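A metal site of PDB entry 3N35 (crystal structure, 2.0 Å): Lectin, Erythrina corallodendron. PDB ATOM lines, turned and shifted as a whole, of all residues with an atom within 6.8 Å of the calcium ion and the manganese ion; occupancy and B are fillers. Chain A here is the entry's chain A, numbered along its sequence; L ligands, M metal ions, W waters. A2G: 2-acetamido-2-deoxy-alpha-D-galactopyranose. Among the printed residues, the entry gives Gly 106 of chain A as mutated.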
ATOM      1  N   ASP A  89      13.932   4.533 -15.712  1.00  0.00           N
ATOM      2  CA  ASP A  89      15.151   4.204 -14.975  1.00  0.00           C
ATOM      3  C   ASP A  89      16.416   4.626 -15.737  1.00  0.00           C
ATOM      4  O   ASP A  89      17.476   4.831 -15.141  1.00  0.00           O
ATOM      5  CB  ASP A  89      15.222   2.706 -14.696  1.00  0.00           C
ATOM      6  CG  ASP A  89      14.612   2.338 -13.362  1.00  0.00           C
ATOM      7  OD1 ASP A  89      15.211   2.685 -12.321  1.00  0.00           O
ATOM      8  OD2 ASP A  89      13.531   1.715 -13.353  1.00  0.00           O
ATOM      9  N   GLY A 106      13.783  -2.358 -14.832  1.00  0.00           N
ATOM     10  CA  GLY A 106      13.916  -1.426 -13.726  1.00  0.00           C
ATOM     11  C   GLY A 106      15.327  -0.886 -13.613  1.00  0.00           C
ATOM     12  O   GLY A 106      15.961  -0.550 -14.620  1.00  0.00           O
ATOM     13  N   GLY A 107      15.843  -0.807 -12.390  1.00  0.00           N
ATOM     14  CA  GLY A 107      17.179  -0.297 -12.153  1.00  0.00           C
ATOM     15  C   GLY A 107      18.313  -1.110 -12.761  1.00  0.00           C
ATOM     16  O   GLY A 107      19.458  -0.655 -12.767  1.00  0.00           O
ATOM     17  N   TYR A 108      18.014  -2.313 -13.239  1.00  0.00           N
ATOM     18  CA  TYR A 108      19.035  -3.175 -13.839  1.00  0.00           C
ATOM     19  C   TYR A 108      19.178  -2.906 -15.335  1.00  0.00           C
ATOM     20  O   TYR A 108      19.995  -3.533 -16.027  1.00  0.00           O
ATOM     21  CB  TYR A 108      18.692  -4.641 -13.580  1.00  0.00           C
ATOM     22  CG  TYR A 108      18.684  -4.950 -12.095  1.00  0.00           C
ATOM     23  CD1 TYR A 108      19.829  -4.792 -11.317  1.00  0.00           C
ATOM     24  CD2 TYR A 108      17.507  -5.355 -11.448  1.00  0.00           C
ATOM     25  CE1 TYR A 108      19.817  -5.016  -9.937  1.00  0.00           C
ATOM     26  CE2 TYR A 108      17.485  -5.589 -10.068  1.00  0.00           C
ATOM     27  CZ  TYR A 108      18.643  -5.412  -9.329  1.00  0.00           C
ATOM     28  OH  TYR A 108      18.618  -5.614  -7.968  1.00  0.00           O
ATOM     29  N   LEU A 109      18.365  -1.975 -15.816  1.00  0.00           N
ATOM     30  CA  LEU A 109      18.374  -1.504 -17.199  1.00  0.00           C
ATOM     31  C   LEU A 109      18.288  -2.549 -18.310  1.00  0.00           C
ATOM     32  O   LEU A 109      18.666  -2.269 -19.458  1.00  0.00           O
ATOM     33  CB  LEU A 109      19.617  -0.629 -17.420  1.00  0.00           C
ATOM     34  CG  LEU A 109      19.739   0.512 -16.411  1.00  0.00           C
ATOM     35  CD1 LEU A 109      21.042   1.272 -16.639  1.00  0.00           C
ATOM     36  CD2 LEU A 109      18.535   1.442 -16.537  1.00  0.00           C
ATOM     37  N   GLU A 127      25.966   3.736 -19.219  1.00  0.00           N
ATOM     38  CA  GLU A 127      24.602   4.102 -18.862  1.00  0.00           C
ATOM     39  C   GLU A 127      24.335   5.588 -18.699  1.00  0.00           C
ATOM     40  O   GLU A 127      25.232   6.386 -18.411  1.00  0.00           O
ATOM     41  CB  GLU A 127      24.226   3.426 -17.551  1.00  0.00           C
ATOM     42  CG  GLU A 127      25.129   3.861 -16.394  1.00  0.00           C
ATOM     43  CD  GLU A 127      24.672   3.348 -15.042  1.00  0.00           C
ATOM     44  OE1 GLU A 127      24.425   2.136 -14.910  1.00  0.00           O
ATOM     45  OE2 GLU A 127      24.554   4.173 -14.114  1.00  0.00           O
ATOM     46  N   ASP A 129      21.797   7.007 -16.322  1.00  0.00           N
ATOM     47  CA  ASP A 129      20.933   6.654 -15.218  1.00  0.00           C
ATOM     48  C   ASP A 129      20.087   7.789 -14.646  1.00  0.00           C
ATOM     49  O   ASP A 129      20.644   8.777 -14.180  1.00  0.00           O
ATOM     50  CB  ASP A 129      21.821   6.081 -14.134  1.00  0.00           C
ATOM     51  CG  ASP A 129      21.086   5.210 -13.183  1.00  0.00           C
ATOM     52  OD1 ASP A 129      19.869   5.433 -12.989  1.00  0.00           O
ATOM     53  OD2 ASP A 129      21.728   4.303 -12.612  1.00  0.00           O
ATOM     54  N   THR A 130      18.770   7.566 -14.665  1.00  0.00           N
ATOM     55  CA  THR A 130      17.878   8.611 -14.160  1.00  0.00           C
ATOM     56  C   THR A 130      17.259   8.426 -12.773  1.00  0.00           C
ATOM     57  O   THR A 130      16.616   9.342 -12.277  1.00  0.00           O
ATOM     58  CB  THR A 130      16.713   8.867 -15.144  1.00  0.00           C
ATOM     59  OG1 THR A 130      16.033   7.638 -15.395  1.00  0.00           O
ATOM     60  CG2 THR A 130      17.233   9.437 -16.461  1.00  0.00           C
ATOM     61  N   PHE A 131      17.440   7.262 -12.153  1.00  0.00           N
ATOM     62  CA  PHE A 131      16.861   7.011 -10.834  1.00  0.00           C
ATOM     63  C   PHE A 131      17.931   6.524  -9.884  1.00  0.00           C
ATOM     64  O   PHE A 131      18.696   5.644 -10.225  1.00  0.00           O
ATOM     65  CB  PHE A 131      15.771   5.933 -10.928  1.00  0.00           C
ATOM     66  CG  PHE A 131      15.097   5.656  -9.619  1.00  0.00           C
ATOM     67  CD1 PHE A 131      14.008   6.412  -9.197  1.00  0.00           C
ATOM     68  CD2 PHE A 131      15.562   4.625  -8.785  1.00  0.00           C
ATOM     69  CE1 PHE A 131      13.395   6.167  -7.961  1.00  0.00           C
ATOM     70  CE2 PHE A 131      14.956   4.383  -7.556  1.00  0.00           C
ATOM     71  CZ  PHE A 131      13.870   5.156  -7.138  1.00  0.00           C
ATOM     72  N   SER A 132      17.994   7.072  -8.674  1.00  0.00           N
ATOM     73  CA  SER A 132      19.019   6.648  -7.727  1.00  0.00           C
ATOM     74  C   SER A 132      18.662   5.403  -6.909  1.00  0.00           C
ATOM     75  O   SER A 132      17.922   5.490  -5.931  1.00  0.00           O
ATOM     76  CB  SER A 132      19.362   7.805  -6.779  1.00  0.00           C
ATOM     77  OG  SER A 132      20.445   7.474  -5.924  1.00  0.00           O
ATOM     78  N   ASN A 133      19.185   4.246  -7.314  1.00  0.00           N
ATOM     79  CA  ASN A 133      18.940   3.004  -6.575  1.00  0.00           C
ATOM     80  C   ASN A 133      19.890   2.946  -5.380  1.00  0.00           C
ATOM     81  O   ASN A 133      20.740   3.811  -5.205  1.00  0.00           O
ATOM     82  CB  ASN A 133      19.150   1.780  -7.462  1.00  0.00           C
ATOM     83  CG  ASN A 133      18.125   1.673  -8.571  1.00  0.00           C
ATOM     84  OD1 ASN A 133      18.316   2.215  -9.650  1.00  0.00           O
ATOM     85  ND2 ASN A 133      17.020   0.987  -8.304  1.00  0.00           N
ATOM     86  N   TRP A 135      22.424   1.222  -4.901  1.00  0.00           N
ATOM     87  CA  TRP A 135      23.818   1.052  -5.298  1.00  0.00           C
ATOM     88  C   TRP A 135      24.333   2.273  -6.063  1.00  0.00           C
ATOM     89  O   TRP A 135      25.498   2.321  -6.463  1.00  0.00           O
ATOM     90  CB  TRP A 135      23.961  -0.177  -6.183  1.00  0.00           C
ATOM     91  CG  TRP A 135      23.073  -0.128  -7.393  1.00  0.00           C
ATOM     92  CD1 TRP A 135      23.266   0.619  -8.523  1.00  0.00           C
ATOM     93  CD2 TRP A 135      21.842  -0.827  -7.577  1.00  0.00           C
ATOM     94  NE1 TRP A 135      22.216   0.432  -9.401  1.00  0.00           N
ATOM     95  CE2 TRP A 135      21.326  -0.457  -8.838  1.00  0.00           C
ATOM     96  CE3 TRP A 135      21.103  -1.728  -6.788  1.00  0.00           C
ATOM     97  CZ2 TRP A 135      20.119  -0.955  -9.336  1.00  0.00           C
ATOM     98  CZ3 TRP A 135      19.905  -2.226  -7.276  1.00  0.00           C
ATOM     99  CH2 TRP A 135      19.423  -1.838  -8.539  1.00  0.00           C
ATOM    100  N   ASP A 136      23.468   3.255  -6.259  1.00  0.00           N
ATOM    101  CA  ASP A 136      23.820   4.453  -6.995  1.00  0.00           C
ATOM    102  C   ASP A 136      24.285   5.625  -6.172  1.00  0.00           C
ATOM    103  O   ASP A 136      24.067   5.679  -4.960  1.00  0.00           O
ATOM    104  CB  ASP A 136      22.630   4.981  -7.788  1.00  0.00           C
ATOM    105  CG  ASP A 136      22.362   4.199  -9.031  1.00  0.00           C
ATOM    106  OD1 ASP A 136      23.318   3.712  -9.655  1.00  0.00           O
ATOM    107  OD2 ASP A 136      21.181   4.102  -9.389  1.00  0.00           O
ATOM    108  N   PRO A 137      24.943   6.590  -6.829  1.00  0.00           N
ATOM    109  CA  PRO A 137      25.374   7.767  -6.089  1.00  0.00           C
ATOM    110  C   PRO A 137      24.056   8.535  -5.965  1.00  0.00           C
ATOM    111  O   PRO A 137      23.112   8.273  -6.714  1.00  0.00           O
ATOM    112  CB  PRO A 137      26.363   8.437  -7.050  1.00  0.00           C
ATOM    113  CG  PRO A 137      25.929   7.954  -8.420  1.00  0.00           C
ATOM    114  CD  PRO A 137      25.584   6.508  -8.152  1.00  0.00           C
ATOM    115  N   VAL A 140      21.365  12.229  -9.706  1.00  0.00           N
ATOM    116  CA  VAL A 140      20.805  11.705 -10.937  1.00  0.00           C
ATOM    117  C   VAL A 140      20.275  12.893 -11.715  1.00  0.00           C
ATOM    118  O   VAL A 140      19.813  13.869 -11.128  1.00  0.00           O
ATOM    119  CB  VAL A 140      19.663  10.686 -10.710  1.00  0.00           C
ATOM    120  CG1 VAL A 140      20.236   9.342 -10.313  1.00  0.00           C
ATOM    121  CG2 VAL A 140      18.704  11.203  -9.645  1.00  0.00           C
ATOM    122  N   HIS A 142      23.031  10.506 -14.059  1.00  0.00           N
ATOM    123  CA  HIS A 142      24.472  10.379 -14.097  1.00  0.00           C
ATOM    124  C   HIS A 142      24.890   9.401 -15.179  1.00  0.00           C
ATOM    125  O   HIS A 142      24.127   8.518 -15.568  1.00  0.00           O
ATOM    126  CB  HIS A 142      25.047   9.921 -12.750  1.00  0.00           C
ATOM    127  CG  HIS A 142      24.519   8.604 -12.257  1.00  0.00           C
ATOM    128  ND1 HIS A 142      23.516   8.504 -11.321  1.00  0.00           N
ATOM    129  CD2 HIS A 142      24.852   7.334 -12.584  1.00  0.00           C
ATOM    130  CE1 HIS A 142      23.266   7.233 -11.079  1.00  0.00           C
ATOM    131  NE2 HIS A 142      24.064   6.499 -11.832  1.00  0.00           N
ATOM    132  N   ILE A 143      26.093   9.602 -15.696  1.00  0.00           N
ATOM    133  CA  ILE A 143      26.653   8.711 -16.701  1.00  0.00           C
ATOM    134  C   ILE A 143      27.449   7.736 -15.848  1.00  0.00           C
ATOM    135  O   ILE A 143      28.037   8.124 -14.847  1.00  0.00           O
ATOM    136  CB  ILE A 143      27.641   9.419 -17.627  1.00  0.00           C
ATOM    137  CG1 ILE A 143      26.970  10.630 -18.266  1.00  0.00           C
ATOM    138  CG2 ILE A 143      28.133   8.440 -18.707  1.00  0.00           C
ATOM    139  CD1 ILE A 143      27.922  11.618 -18.945  1.00  0.00           C
ATOM    140  N   GLY A 144      27.480   6.472 -16.242  1.00  0.00           N
ATOM    141  CA  GLY A 144      28.238   5.515 -15.470  1.00  0.00           C
ATOM    142  C   GLY A 144      28.904   4.492 -16.361  1.00  0.00           C
ATOM    143  O   GLY A 144      28.397   4.186 -17.437  1.00  0.00           O
ATOM    144  N   ASP A 146      29.814   0.728 -16.464  1.00  0.00           N
ATOM    145  CA  ASP A 146      29.497  -0.511 -15.774  1.00  0.00           C
ATOM    146  C   ASP A 146      30.304  -1.680 -16.311  1.00  0.00           C
ATOM    147  O   ASP A 146      30.244  -2.006 -17.500  1.00  0.00           O
ATOM    148  CB  ASP A 146      28.005  -0.837 -15.916  1.00  0.00           C
ATOM    149  CG  ASP A 146      27.108   0.300 -15.432  1.00  0.00           C
ATOM    150  OD1 ASP A 146      27.610   1.188 -14.715  1.00  0.00           O
ATOM    151  OD2 ASP A 146      25.899   0.286 -15.763  1.00  0.00           O
ATOM    152  N   ILE A 150      25.994  -3.498 -12.106  1.00  0.00           N
ATOM    153  CA  ILE A 150      25.153  -2.317 -12.251  1.00  0.00           C
ATOM    154  C   ILE A 150      25.758  -1.210 -11.386  1.00  0.00           C
ATOM    155  O   ILE A 150      25.446  -0.023 -11.538  1.00  0.00           O
ATOM    156  CB  ILE A 150      23.692  -2.621 -11.823  1.00  0.00           C
ATOM    157  CG1 ILE A 150      22.764  -1.484 -12.264  1.00  0.00           C
ATOM    158  CG2 ILE A 150      23.622  -2.861 -10.326  1.00  0.00           C
ATOM    159  CD1 ILE A 150      22.478  -1.422 -13.760  1.00  0.00           C
ATOM    160  N   ARG A 151      26.619  -1.606 -10.448  1.00  0.00           N
ATOM    161  CA  ARG A 151      27.297  -0.667  -9.570  1.00  0.00           C
ATOM    162  C   ARG A 151      28.520  -0.184 -10.365  1.00  0.00           C
ATOM    163  O   ARG A 151      29.518  -0.903 -10.487  1.00  0.00           O
ATOM    164  CB  ARG A 151      27.713  -1.371  -8.275  1.00  0.00           C
ATOM    165  CG  ARG A 151      28.399  -0.463  -7.261  1.00  0.00           C
ATOM    166  CD  ARG A 151      28.754  -1.209  -5.959  1.00  0.00           C
ATOM    167  NE  ARG A 151      27.700  -1.165  -4.959  1.00  0.00           N
ATOM    168  CZ  ARG A 151      26.788  -2.119  -4.757  1.00  0.00           C
ATOM    169  NH1 ARG A 151      26.793  -3.213  -5.504  1.00  0.00           N
ATOM    170  NH2 ARG A 151      25.881  -1.980  -3.797  1.00  0.00           N
ATOM    171  N   SER A 152      28.427   1.021 -10.913  1.00  0.00           N
ATOM    172  CA  SER A 152      29.489   1.599 -11.744  1.00  0.00           C
ATOM    173  C   SER A 152      30.851   1.730 -11.085  1.00  0.00           C
ATOM    174  O   SER A 152      30.953   1.969  -9.880  1.00  0.00           O
ATOM    175  CB  SER A 152      29.046   2.978 -12.246  1.00  0.00           C
ATOM    176  OG  SER A 152      27.749   2.938 -12.817  1.00  0.00           O
ATOM    177  N   THR A 155      31.286   7.273 -12.116  1.00  0.00           N
ATOM    178  CA  THR A 155      30.095   8.004 -12.520  1.00  0.00           C
ATOM    179  C   THR A 155      30.371   9.493 -12.684  1.00  0.00           C
ATOM    180  O   THR A 155      31.331  10.027 -12.126  1.00  0.00           O
ATOM    181  CB  THR A 155      28.951   7.840 -11.504  1.00  0.00           C
ATOM    182  OG1 THR A 155      29.358   8.333 -10.223  1.00  0.00           O
ATOM    183  CG2 THR A 155      28.558   6.378 -11.380  1.00  0.00           C
HETATM  184  O5  A2G L   1      11.072   1.094  -8.745  1.00  0.00           O
HETATM  185  C1  A2G L   1      11.955   0.151  -8.128  1.00  0.00           C
HETATM  186  O1  A2G L   1      12.364   0.690  -6.851  1.00  0.00           O
HETATM  187  C2  A2G L   1      13.165  -0.034  -9.056  1.00  0.00           C
HETATM  188  N2  A2G L   1      14.138  -0.850  -8.337  1.00  0.00           N
HETATM  189  C3  A2G L   1      13.843   1.320  -9.316  1.00  0.00           C
HETATM  190  O3  A2G L   1      14.859   1.165 -10.304  1.00  0.00           O
HETATM  191  C4  A2G L   1      12.824   2.349  -9.803  1.00  0.00           C
HETATM  192  O4  A2G L   1      12.348   1.941 -11.086  1.00  0.00           O
HETATM  193  C5  A2G L   1      11.639   2.401  -8.850  1.00  0.00           C
HETATM  194  C6  A2G L   1      10.559   3.361  -9.346  1.00  0.00           C
HETATM  195  O6  A2G L   1      10.104   4.070  -8.205  1.00  0.00           O
HETATM  196  C7  A2G L   1      14.769  -1.879  -8.937  1.00  0.00           C
HETATM  197  O7  A2G L   1      14.576  -2.187 -10.106  1.00  0.00           O
HETATM  198  C8  A2G L   1      15.744  -2.643  -8.092  1.00  0.00           C
HETATM  199 CA    CA M   1      19.702   3.609 -11.223  1.00  0.00          CA
HETATM  200 MN    MN M   2      23.921   4.170 -11.887  1.00  0.00          MN
HETATM  201  O   HOH W   1      20.818   1.417 -12.082  1.00  0.00           O
HETATM  202  O   HOH W   2      23.647   1.828 -12.192  1.00  0.00           O
HETATM  203  O   HOH W   3      26.158   3.897 -11.059  1.00  0.00           O
HETATM  204  O   HOH W   4      17.716   3.281 -12.921  1.00  0.00           O
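The side-chain amide nitrogen (ND2) of Asn 133 lies within hydrogen-bond range of an oxygen (O3) of the ligand, 2.9 Å away. N of Gly 107 lies within hydrogen-bond range of O7 of the ligand, at 3.0 Å. The side-chain carboxylate of Asp 89 is in hydrogen-bond range of an oxygen (O3) of the ligand, 2.6 Å away.
The side-chain carboxylate of Glu 127 sits close to the side-chain carboxylate of Asp 146 (2.5 Å). The backbone NH (N) of Glu 127 lies within hydrogen-bond range of the backbone carbonyl oxygen (O) of Gly 144 (3.0 Å). The indole nitrogen of Trp 135 sits close to the side-chain carboxylate of Asp 136, 3.5 Å away.
Of the 23 residues printed, 4 come within 4 Å of the manganese ion.
The calcium ion is bound by the side-chain carboxylate (OD2) of Asp 136 (2.4 Å), the backbone carbonyl oxygen (O) of Phe 131 (2.5 Å), the side-chain amide oxygen (OD1) of Asn 133 (2.5 Å), the side-chain carboxylate (OD1) of Asp 129 (2.5 Å), the side-chain carboxylate (OD2) of Asp 129 (2.6 Å), water W1 (2.6 Å) and water W4 (2.6 Å).
The manganese ion is bound by OD2 of Asp 129 (2.3 Å), OE2 of Glu 127 (2.3 Å), NE2 of His 142 (2.3 Å), OD1 of Asp 136 (2.4 Å), water W2 (2.4 Å) and water W3 (2.4 Å). The manganese ion has six donor atoms within binding distance.
Water W1 lies within hydrogen-bond range of O of Gly 107 (2.6 Å) and NE1 of Trp 135 (3.2 Å). Water W2 lies within hydrogen-bond range of the backbone carbonyl oxygen of Ile 150 (2.7 Å), the side-chain carboxylate of Glu 127 (2.8 Å) and the indole nitrogen of Trp 135 (3.4 Å).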
